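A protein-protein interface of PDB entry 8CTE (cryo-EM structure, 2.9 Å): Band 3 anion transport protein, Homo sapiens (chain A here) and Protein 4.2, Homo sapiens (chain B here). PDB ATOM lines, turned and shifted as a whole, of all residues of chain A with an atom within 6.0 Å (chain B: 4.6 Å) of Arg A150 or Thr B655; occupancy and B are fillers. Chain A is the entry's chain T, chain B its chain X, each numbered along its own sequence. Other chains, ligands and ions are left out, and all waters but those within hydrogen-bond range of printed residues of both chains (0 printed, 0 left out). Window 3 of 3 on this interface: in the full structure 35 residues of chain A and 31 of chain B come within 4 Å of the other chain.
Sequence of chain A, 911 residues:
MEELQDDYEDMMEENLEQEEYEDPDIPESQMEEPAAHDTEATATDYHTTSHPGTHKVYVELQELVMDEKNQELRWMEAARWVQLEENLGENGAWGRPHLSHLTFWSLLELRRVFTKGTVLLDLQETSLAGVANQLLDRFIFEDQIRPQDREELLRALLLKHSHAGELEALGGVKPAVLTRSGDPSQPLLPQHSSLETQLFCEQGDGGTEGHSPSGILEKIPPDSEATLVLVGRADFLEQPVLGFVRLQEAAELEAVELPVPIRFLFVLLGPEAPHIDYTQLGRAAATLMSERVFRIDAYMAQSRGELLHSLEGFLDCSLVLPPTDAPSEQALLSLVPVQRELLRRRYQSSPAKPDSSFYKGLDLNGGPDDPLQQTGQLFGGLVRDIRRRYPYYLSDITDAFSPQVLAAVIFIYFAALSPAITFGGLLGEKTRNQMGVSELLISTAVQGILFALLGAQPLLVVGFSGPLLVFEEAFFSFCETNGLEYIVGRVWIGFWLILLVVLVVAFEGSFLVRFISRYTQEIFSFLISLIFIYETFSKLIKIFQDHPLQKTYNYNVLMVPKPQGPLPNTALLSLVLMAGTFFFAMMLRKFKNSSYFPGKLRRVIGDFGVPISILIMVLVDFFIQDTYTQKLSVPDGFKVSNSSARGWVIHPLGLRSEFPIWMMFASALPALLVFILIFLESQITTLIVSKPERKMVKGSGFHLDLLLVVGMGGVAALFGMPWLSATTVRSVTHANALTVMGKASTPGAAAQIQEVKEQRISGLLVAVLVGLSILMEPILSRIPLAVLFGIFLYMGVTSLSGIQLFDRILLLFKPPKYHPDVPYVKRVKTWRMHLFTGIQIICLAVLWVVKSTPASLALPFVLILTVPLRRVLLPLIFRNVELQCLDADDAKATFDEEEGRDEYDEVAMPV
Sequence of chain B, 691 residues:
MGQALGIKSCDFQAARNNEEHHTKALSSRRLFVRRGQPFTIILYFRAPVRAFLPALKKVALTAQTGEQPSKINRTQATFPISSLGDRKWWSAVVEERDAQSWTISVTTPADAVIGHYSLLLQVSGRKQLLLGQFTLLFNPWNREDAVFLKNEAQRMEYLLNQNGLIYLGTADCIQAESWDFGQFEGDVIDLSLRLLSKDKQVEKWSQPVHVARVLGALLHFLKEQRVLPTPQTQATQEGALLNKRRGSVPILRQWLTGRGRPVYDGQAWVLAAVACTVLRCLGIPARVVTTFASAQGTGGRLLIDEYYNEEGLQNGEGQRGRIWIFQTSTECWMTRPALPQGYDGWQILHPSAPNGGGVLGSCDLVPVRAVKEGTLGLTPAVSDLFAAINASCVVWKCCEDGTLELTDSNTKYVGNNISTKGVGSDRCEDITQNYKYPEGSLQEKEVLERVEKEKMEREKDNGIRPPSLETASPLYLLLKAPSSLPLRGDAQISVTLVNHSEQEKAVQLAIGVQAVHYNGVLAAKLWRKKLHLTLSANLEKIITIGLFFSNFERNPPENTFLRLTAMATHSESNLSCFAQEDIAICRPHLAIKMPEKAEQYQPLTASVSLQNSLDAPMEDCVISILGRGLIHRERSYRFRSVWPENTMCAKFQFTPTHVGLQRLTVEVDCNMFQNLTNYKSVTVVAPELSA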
ATOM      1  N   ALA A 132     -23.509 -17.443 -12.009  1.00  0.00           N
ATOM      2  CA  ALA A 132     -24.391 -16.839 -13.004  1.00  0.00           C
ATOM      3  C   ALA A 132     -24.459 -15.325 -12.844  1.00  0.00           C
ATOM      4  O   ALA A 132     -24.429 -14.590 -13.838  1.00  0.00           O
ATOM      5  CB  ALA A 132     -25.787 -17.453 -12.909  1.00  0.00           C
ATOM      6  N   ASN A 133     -24.551 -14.841 -11.602  1.00  0.00           N
ATOM      7  CA  ASN A 133     -24.606 -13.401 -11.367  1.00  0.00           C
ATOM      8  C   ASN A 133     -23.321 -12.715 -11.818  1.00  0.00           C
ATOM      9  O   ASN A 133     -23.365 -11.669 -12.475  1.00  0.00           O
ATOM     10  CB  ASN A 133     -24.874 -13.119  -9.889  1.00  0.00           C
ATOM     11  CG  ASN A 133     -26.293 -13.460  -9.479  1.00  0.00           C
ATOM     12  OD1 ASN A 133     -27.237 -13.254 -10.241  1.00  0.00           O
ATOM     13  ND2 ASN A 133     -26.450 -13.984  -8.269  1.00  0.00           N
ATOM     14  N   GLN A 134     -22.165 -13.297 -11.482  1.00  0.00           N
ATOM     15  CA  GLN A 134     -20.895 -12.712 -11.906  1.00  0.00           C
ATOM     16  C   GLN A 134     -20.751 -12.742 -13.424  1.00  0.00           C
ATOM     17  O   GLN A 134     -20.268 -11.774 -14.026  1.00  0.00           O
ATOM     18  CB  GLN A 134     -19.729 -13.442 -11.240  1.00  0.00           C
ATOM     19  CG  GLN A 134     -19.674 -13.290  -9.725  1.00  0.00           C
ATOM     20  CD  GLN A 134     -19.375 -11.870  -9.283  1.00  0.00           C
ATOM     21  OE1 GLN A 134     -18.759 -11.095 -10.014  1.00  0.00           O
ATOM     22  NE2 GLN A 134     -19.816 -11.522  -8.079  1.00  0.00           N
ATOM     23  N   LEU A 136     -23.190 -12.704 -15.674  1.00  0.00           N
ATOM     24  CA  LEU A 136     -24.076 -11.706 -16.265  1.00  0.00           C
ATOM     25  C   LEU A 136     -23.560 -10.290 -16.034  1.00  0.00           C
ATOM     26  O   LEU A 136     -23.681  -9.433 -16.917  1.00  0.00           O
ATOM     27  CB  LEU A 136     -25.489 -11.864 -15.714  1.00  0.00           C
ATOM     28  CG  LEU A 136     -26.206 -13.138 -16.163  1.00  0.00           C
ATOM     29  CD1 LEU A 136     -27.646 -13.137 -15.688  1.00  0.00           C
ATOM     30  CD2 LEU A 136     -26.133 -13.293 -17.676  1.00  0.00           C
ATOM     31  N   ASP A 137     -22.978 -10.028 -14.858  1.00  0.00           N
ATOM     32  CA  ASP A 137     -22.390  -8.716 -14.607  1.00  0.00           C
ATOM     33  C   ASP A 137     -21.231  -8.439 -15.556  1.00  0.00           C
ATOM     34  O   ASP A 137     -21.099  -7.324 -16.076  1.00  0.00           O
ATOM     35  CB  ASP A 137     -21.933  -8.612 -13.153  1.00  0.00           C
ATOM     36  CG  ASP A 137     -23.093  -8.555 -12.182  1.00  0.00           C
ATOM     37  OD1 ASP A 137     -24.254  -8.610 -12.640  1.00  0.00           O
ATOM     38  OD2 ASP A 137     -22.846  -8.454 -10.962  1.00  0.00           O
ATOM     39  N   ILE A 140     -22.637  -7.715 -19.048  1.00  0.00           N
ATOM     40  CA  ILE A 140     -23.103  -6.339 -19.176  1.00  0.00           C
ATOM     41  C   ILE A 140     -21.921  -5.379 -19.234  1.00  0.00           C
ATOM     42  O   ILE A 140     -21.933  -4.401 -19.994  1.00  0.00           O
ATOM     43  CB  ILE A 140     -24.066  -5.993 -18.026  1.00  0.00           C
ATOM     44  CG1 ILE A 140     -25.315  -6.875 -18.097  1.00  0.00           C
ATOM     45  CG2 ILE A 140     -24.460  -4.524 -18.068  1.00  0.00           C
ATOM     46  CD1 ILE A 140     -26.348  -6.554 -17.044  1.00  0.00           C
ATOM     47  N   ILE A 145     -24.199  -8.583 -23.524  1.00  0.00           N
ATOM     48  CA  ILE A 145     -25.652  -8.581 -23.471  1.00  0.00           C
ATOM     49  C   ILE A 145     -26.118  -7.205 -23.013  1.00  0.00           C
ATOM     50  O   ILE A 145     -25.354  -6.419 -22.452  1.00  0.00           O
ATOM     51  CB  ILE A 145     -26.212  -9.675 -22.536  1.00  0.00           C
ATOM     52  CG1 ILE A 145     -25.840  -9.367 -21.084  1.00  0.00           C
ATOM     53  CG2 ILE A 145     -25.715 -11.053 -22.952  1.00  0.00           C
ATOM     54  CD1 ILE A 145     -26.413 -10.339 -20.082  1.00  0.00           C
ATOM     55  N   ARG A 146     -27.389  -6.922 -23.264  1.00  0.00           N
ATOM     56  CA  ARG A 146     -27.999  -5.692 -22.797  1.00  0.00           C
ATOM     57  C   ARG A 146     -28.461  -5.848 -21.351  1.00  0.00           C
ATOM     58  O   ARG A 146     -28.748  -6.962 -20.902  1.00  0.00           O
ATOM     59  CB  ARG A 146     -29.183  -5.316 -23.690  1.00  0.00           C
ATOM     60  CG  ARG A 146     -28.787  -4.970 -25.117  1.00  0.00           C
ATOM     61  CD  ARG A 146     -30.002  -4.821 -26.016  1.00  0.00           C
ATOM     62  NE  ARG A 146     -30.731  -6.076 -26.156  1.00  0.00           N
ATOM     63  CZ  ARG A 146     -31.784  -6.247 -26.945  1.00  0.00           C
ATOM     64  NH1 ARG A 146     -32.261  -5.260 -27.685  1.00  0.00           N
ATOM     65  NH2 ARG A 146     -32.371  -7.440 -26.992  1.00  0.00           N
ATOM     66  N   PRO A 147     -28.526  -4.750 -20.592  1.00  0.00           N
ATOM     67  CA  PRO A 147     -29.003  -4.848 -19.202  1.00  0.00           C
ATOM     68  C   PRO A 147     -30.430  -5.348 -19.077  1.00  0.00           C
ATOM     69  O   PRO A 147     -30.792  -5.887 -18.023  1.00  0.00           O
ATOM     70  CB  PRO A 147     -28.866  -3.411 -18.681  1.00  0.00           C
ATOM     71  CG  PRO A 147     -27.820  -2.795 -19.547  1.00  0.00           C
ATOM     72  CD  PRO A 147     -28.013  -3.405 -20.903  1.00  0.00           C
ATOM     73  N   GLN A 148     -31.254  -5.186 -20.113  1.00  0.00           N
ATOM     74  CA  GLN A 148     -32.626  -5.674 -20.073  1.00  0.00           C
ATOM     75  C   GLN A 148     -32.721  -7.186 -20.234  1.00  0.00           C
ATOM     76  O   GLN A 148     -33.769  -7.761 -19.917  1.00  0.00           O
ATOM     77  CB  GLN A 148     -33.457  -4.979 -21.155  1.00  0.00           C
ATOM     78  CG  GLN A 148     -32.794  -4.952 -22.524  1.00  0.00           C
ATOM     79  CD  GLN A 148     -33.683  -4.354 -23.597  1.00  0.00           C
ATOM     80  OE1 GLN A 148     -34.870  -4.115 -23.375  1.00  0.00           O
ATOM     81  NE2 GLN A 148     -33.111  -4.108 -24.770  1.00  0.00           N
ATOM     82  N   ASP A 149     -31.663  -7.841 -20.716  1.00  0.00           N
ATOM     83  CA  ASP A 149     -31.655  -9.290 -20.880  1.00  0.00           C
ATOM     84  C   ASP A 149     -31.143 -10.028 -19.649  1.00  0.00           C
ATOM     85  O   ASP A 149     -31.198 -11.265 -19.623  1.00  0.00           O
ATOM     86  CB  ASP A 149     -30.796  -9.677 -22.087  1.00  0.00           C
ATOM     87  CG  ASP A 149     -31.160  -8.903 -23.337  1.00  0.00           C
ATOM     88  OD1 ASP A 149     -32.118  -8.105 -23.286  1.00  0.00           O
ATOM     89  OD2 ASP A 149     -30.485  -9.090 -24.371  1.00  0.00           O
ATOM     90  N   ARG A 150     -30.645  -9.302 -18.643  1.00  0.00           N
ATOM     91  CA  ARG A 150     -30.018  -9.947 -17.493  1.00  0.00           C
ATOM     92  C   ARG A 150     -31.018 -10.771 -16.694  1.00  0.00           C
ATOM     93  O   ARG A 150     -30.692 -11.870 -16.234  1.00  0.00           O
ATOM     94  CB  ARG A 150     -29.356  -8.902 -16.595  1.00  0.00           C
ATOM     95  CG  ARG A 150     -28.501  -9.503 -15.492  1.00  0.00           C
ATOM     96  CD  ARG A 150     -28.096  -8.472 -14.454  1.00  0.00           C
ATOM     97  NE  ARG A 150     -27.142  -9.019 -13.497  1.00  0.00           N
ATOM     98  CZ  ARG A 150     -27.477  -9.716 -12.420  1.00  0.00           C
ATOM     99  NH1 ARG A 150     -28.742  -9.965 -12.124  1.00  0.00           N
ATOM    100  NH2 ARG A 150     -26.518 -10.176 -11.622  1.00  0.00           N
ATOM    101  N   GLU A 151     -32.235 -10.254 -16.507  1.00  0.00           N
ATOM    102  CA  GLU A 151     -33.236 -10.978 -15.728  1.00  0.00           C
ATOM    103  C   GLU A 151     -33.630 -12.281 -16.413  1.00  0.00           C
ATOM    104  O   GLU A 151     -33.729 -13.331 -15.765  1.00  0.00           O
ATOM    105  CB  GLU A 151     -34.460 -10.089 -15.500  1.00  0.00           C
ATOM    106  CG  GLU A 151     -35.386 -10.552 -14.382  1.00  0.00           C
ATOM    107  CD  GLU A 151     -36.403 -11.582 -14.840  1.00  0.00           C
ATOM    108  OE1 GLU A 151     -36.642 -11.683 -16.062  1.00  0.00           O
ATOM    109  OE2 GLU A 151     -36.963 -12.291 -13.977  1.00  0.00           O
ATOM    110  N   GLU A 152     -33.850 -12.235 -17.730  1.00  0.00           N
ATOM    111  CA  GLU A 152     -34.209 -13.442 -18.469  1.00  0.00           C
ATOM    112  C   GLU A 152     -33.076 -14.460 -18.456  1.00  0.00           C
ATOM    113  O   GLU A 152     -33.316 -15.661 -18.279  1.00  0.00           O
ATOM    114  CB  GLU A 152     -34.590 -13.086 -19.905  1.00  0.00           C
ATOM    115  CG  GLU A 152     -35.853 -12.244 -20.043  1.00  0.00           C
ATOM    116  CD  GLU A 152     -35.597 -10.751 -19.917  1.00  0.00           C
ATOM    117  OE1 GLU A 152     -34.679 -10.356 -19.168  1.00  0.00           O
ATOM    118  OE2 GLU A 152     -36.316  -9.969 -20.576  1.00  0.00           O
ATOM    119  N   LEU A 153     -31.834 -14.004 -18.637  1.00  0.00           N
ATOM    120  CA  LEU A 153     -30.712 -14.936 -18.623  1.00  0.00           C
ATOM    121  C   LEU A 153     -30.493 -15.529 -17.236  1.00  0.00           C
ATOM    122  O   LEU A 153     -30.129 -16.704 -17.115  1.00  0.00           O
ATOM    123  CB  LEU A 153     -29.444 -14.249 -19.127  1.00  0.00           C
ATOM    124  CG  LEU A 153     -29.433 -13.915 -20.622  1.00  0.00           C
ATOM    125  CD1 LEU A 153     -28.046 -13.489 -21.075  1.00  0.00           C
ATOM    126  CD2 LEU A 153     -29.935 -15.092 -21.453  1.00  0.00           C
ATOM    127  N   LEU A 154     -30.710 -14.739 -16.181  1.00  0.00           N
ATOM    128  CA  LEU A 154     -30.599 -15.268 -14.825  1.00  0.00           C
ATOM    129  C   LEU A 154     -31.697 -16.283 -14.539  1.00  0.00           C
ATOM    130  O   LEU A 154     -31.461 -17.286 -13.856  1.00  0.00           O
ATOM    131  CB  LEU A 154     -30.644 -14.124 -13.811  1.00  0.00           C
ATOM    132  CG  LEU A 154     -30.354 -14.501 -12.359  1.00  0.00           C
ATOM    133  CD1 LEU A 154     -28.997 -15.181 -12.246  1.00  0.00           C
ATOM    134  CD2 LEU A 154     -30.420 -13.276 -11.461  1.00  0.00           C
ATOM    135  N   ARG A 155     -32.908 -16.033 -15.045  1.00  0.00           N
ATOM    136  CA  ARG A 155     -33.982 -17.011 -14.911  1.00  0.00           C
ATOM    137  C   ARG A 155     -33.644 -18.304 -15.643  1.00  0.00           C
ATOM    138  O   ARG A 155     -33.885 -19.401 -15.127  1.00  0.00           O
ATOM    139  CB  ARG A 155     -35.291 -16.418 -15.435  1.00  0.00           C
ATOM    140  CG  ARG A 155     -36.407 -17.427 -15.661  1.00  0.00           C
ATOM    141  CD  ARG A 155     -36.890 -18.046 -14.360  1.00  0.00           C
ATOM    142  NE  ARG A 155     -37.955 -19.015 -14.591  1.00  0.00           N
ATOM    143  CZ  ARG A 155     -38.563 -19.703 -13.634  1.00  0.00           C
ATOM    144  NH1 ARG A 155     -38.238 -19.553 -12.360  1.00  0.00           N
ATOM    145  NH2 ARG A 155     -39.523 -20.563 -13.964  1.00  0.00           N
ATOM    146  N   TYR B 601     -27.851 -12.707  -3.892  1.00  0.00           N
ATOM    147  CA  TYR B 601     -28.334 -13.107  -5.212  1.00  0.00           C
ATOM    148  C   TYR B 601     -29.403 -12.170  -5.756  1.00  0.00           C
ATOM    149  O   TYR B 601     -30.193 -12.577  -6.618  1.00  0.00           O
ATOM    150  CB  TYR B 601     -28.863 -14.547  -5.217  1.00  0.00           C
ATOM    151  CG  TYR B 601     -27.858 -15.569  -4.735  1.00  0.00           C
ATOM    152  CD1 TYR B 601     -26.502 -15.418  -4.995  1.00  0.00           C
ATOM    153  CD2 TYR B 601     -28.266 -16.683  -4.015  1.00  0.00           C
ATOM    154  CE1 TYR B 601     -25.582 -16.350  -4.555  1.00  0.00           C
ATOM    155  CE2 TYR B 601     -27.356 -17.619  -3.571  1.00  0.00           C
ATOM    156  CZ  TYR B 601     -26.015 -17.450  -3.844  1.00  0.00           C
ATOM    157  OH  TYR B 601     -25.103 -18.381  -3.404  1.00  0.00           O
ATOM    158  N   GLN B 602     -29.454 -10.927  -5.281  1.00  0.00           N
ATOM    159  CA  GLN B 602     -30.366  -9.909  -5.768  1.00  0.00           C
ATOM    160  C   GLN B 602     -29.588  -8.672  -6.201  1.00  0.00           C
ATOM    161  O   GLN B 602     -28.557  -8.354  -5.599  1.00  0.00           O
ATOM    162  CB  GLN B 602     -31.386  -9.521  -4.691  1.00  0.00           C
ATOM    163  CG  GLN B 602     -32.282 -10.665  -4.241  1.00  0.00           C
ATOM    164  CD  GLN B 602     -33.182 -11.178  -5.349  1.00  0.00           C
ATOM    165  OE1 GLN B 602     -33.552 -10.437  -6.260  1.00  0.00           O
ATOM    166  NE2 GLN B 602     -33.537 -12.455  -5.277  1.00  0.00           N
ATOM    167  N   PRO B 603     -30.041  -7.970  -7.240  1.00  0.00           N
ATOM    168  CA  PRO B 603     -29.299  -6.794  -7.709  1.00  0.00           C
ATOM    169  C   PRO B 603     -29.255  -5.692  -6.662  1.00  0.00           C
ATOM    170  O   PRO B 603     -30.238  -5.425  -5.967  1.00  0.00           O
ATOM    171  CB  PRO B 603     -30.080  -6.353  -8.954  1.00  0.00           C
ATOM    172  CG  PRO B 603     -31.447  -6.930  -8.771  1.00  0.00           C
ATOM    173  CD  PRO B 603     -31.236  -8.232  -8.061  1.00  0.00           C
ATOM    174  N   LEU B 604     -28.096  -5.046  -6.563  1.00  0.00           N
ATOM    175  CA  LEU B 604     -27.875  -3.943  -5.642  1.00  0.00           C
ATOM    176  C   LEU B 604     -27.327  -2.756  -6.417  1.00  0.00           C
ATOM    177  O   LEU B 604     -26.449  -2.914  -7.271  1.00  0.00           O
ATOM    178  CB  LEU B 604     -26.907  -4.337  -4.519  1.00  0.00           C
ATOM    179  CG  LEU B 604     -26.593  -3.279  -3.463  1.00  0.00           C
ATOM    180  CD1 LEU B 604     -27.842  -2.926  -2.675  1.00  0.00           C
ATOM    181  CD2 LEU B 604     -25.489  -3.752  -2.535  1.00  0.00           C
ATOM    182  N   LEU B 630     -18.364  -9.024  -3.414  1.00  0.00           N
ATOM    183  CA  LEU B 630     -19.321  -8.236  -4.179  1.00  0.00           C
ATOM    184  C   LEU B 630     -19.004  -8.222  -5.664  1.00  0.00           C
ATOM    185  O   LEU B 630     -19.892  -8.475  -6.486  1.00  0.00           O
ATOM    186  CB  LEU B 630     -19.366  -6.792  -3.647  1.00  0.00           C
ATOM    187  CG  LEU B 630     -19.816  -6.583  -2.201  1.00  0.00           C
ATOM    188  CD1 LEU B 630     -19.771  -5.110  -1.835  1.00  0.00           C
ATOM    189  CD2 LEU B 630     -21.209  -7.145  -1.990  1.00  0.00           C
ATOM    190  N   PHE B 654     -24.845  -4.090  -9.232  1.00  0.00           N
ATOM    191  CA  PHE B 654     -24.120  -5.342  -9.079  1.00  0.00           C
ATOM    192  C   PHE B 654     -24.883  -6.228  -8.107  1.00  0.00           C
ATOM    193  O   PHE B 654     -25.687  -5.752  -7.301  1.00  0.00           O
ATOM    194  CB  PHE B 654     -22.680  -5.109  -8.599  1.00  0.00           C
ATOM    195  CG  PHE B 654     -22.579  -4.339  -7.310  1.00  0.00           C
ATOM    196  CD1 PHE B 654     -22.515  -5.000  -6.094  1.00  0.00           C
ATOM    197  CD2 PHE B 654     -22.537  -2.953  -7.316  1.00  0.00           C
ATOM    198  CE1 PHE B 654     -22.421  -4.295  -4.909  1.00  0.00           C
ATOM    199  CE2 PHE B 654     -22.442  -2.243  -6.134  1.00  0.00           C
ATOM    200  CZ  PHE B 654     -22.384  -2.915  -4.929  1.00  0.00           C
ATOM    201  N   THR B 655     -24.622  -7.531  -8.191  1.00  0.00           N
ATOM    202  CA  THR B 655     -25.340  -8.508  -7.386  1.00  0.00           C
ATOM    203  C   THR B 655     -24.413  -9.102  -6.339  1.00  0.00           C
ATOM    204  O   THR B 655     -23.457  -9.808  -6.697  1.00  0.00           O
ATOM    205  CB  THR B 655     -25.919  -9.612  -8.270  1.00  0.00           C
ATOM    206  OG1 THR B 655     -26.810  -9.036  -9.236  1.00  0.00           O
ATOM    207  CG2 THR B 655     -26.679 -10.617  -7.426  1.00  0.00           C
ATOM    208  N   PRO B 656     -24.636  -8.832  -5.053  1.00  0.00           N
ATOM    209  CA  PRO B 656     -23.859  -9.512  -4.008  1.00  0.00           C
ATOM    210  C   PRO B 656     -24.096 -11.014  -4.037  1.00  0.00           C
ATOM    211  O   PRO B 656     -25.208 -11.481  -4.289  1.00  0.00           O
ATOM    212  CB  PRO B 656     -24.381  -8.883  -2.712  1.00  0.00           C
ATOM    213  CG  PRO B 656     -24.954  -7.569  -3.130  1.00  0.00           C
ATOM    214  CD  PRO B 656     -25.525  -7.799  -4.496  1.00  0.00           C
ATOM    215  N   THR B 657     -23.033 -11.773  -3.768  1.00  0.00           N
ATOM    216  CA  THR B 657     -23.093 -13.225  -3.811  1.00  0.00           C
ATOM    217  C   THR B 657     -22.587 -13.909  -2.549  1.00  0.00           C
ATOM    218  O   THR B 657     -22.719 -15.133  -2.441  1.00  0.00           O
ATOM    219  CB  THR B 657     -22.295 -13.762  -5.012  1.00  0.00           C
ATOM    220  OG1 THR B 657     -20.936 -13.314  -4.927  1.00  0.00           O
ATOM    221  CG2 THR B 657     -22.905 -13.283  -6.323  1.00  0.00           C
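Of the 9 printed residues of chain B, 5 touch a printed residue of chain A.
Printed residues of chain B that touch a printed residue of chain A: Tyr B601, Leu B630, Phe B654, Thr B655 and Thr B657.
Printed residues of chain A that touch a printed residue of chain B: Asn A133, Gln A134, Asp A137 and Arg A150.
Along chain A the printed residues that touch a printed residue of chain B span positions 133 to 150.
Among the printed residues, no Asp or Glu carboxylate lies within 4 Å of a Lys or Arg side-chain nitrogen of the other chain.
NE2 of Gln A134 lies within hydrogen-bond range of O of Leu B630 (3.4 Å).
OG1 of Thr B655 sits at hydrogen-bond distance from NH2 of Arg A150, at 2.7 Å.
The side-chain carboxylate (OD2) of Asp A137 sits at hydrogen-bond distance from the backbone NH (N) of Thr B655 (3.4 Å).
ND2 of Asn A133 touches CD1 of Tyr B601 (3.6 Å).
Asn A133 touches Thr B655.
Thr B657 touches Gln A134.
Phe B654 touches Asp A137.
Of chain B, only Thr B655 (2.7 Å) comes within 4 Å of Arg A150.
Of the printed residues of chain B, Asn A133 touches Tyr B601 (3.6 Å) and Thr B655 (3.5 Å).
Of the printed residues of chain A, Leu B630 touches Gln A134 (3.4 Å).
Printed residues of chain A within 4 Å of Thr B657: Gln A134.
Printed residues of chain A within 4 Å of Phe B654: Asp A137.
Printed residues of chain A within 4 Å of Tyr B601: Asn A133 (3.6 Å).
Gln B602 touches none of the printed residues of chain A.
Leu B604 touches none of the printed residues of chain A.
The nearest residue of chain A that does not touch Thr B655 is Gln A134 (4.3 Å).
NH2 of Arg A150 sits at hydrogen-bond distance from OD1 of Asn A133 (3.4 Å).
The backbone carbonyl oxygen (O) of Pro B656 sits at hydrogen-bond distance from the backbone NH (N) of Tyr B601.
OD1 of Asp A137 is in salt-bridge range of NH2 of Arg A150, 2.9 Å away.
N of Leu B604 sits at hydrogen-bond distance from O of Phe B654 (2.6 Å).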
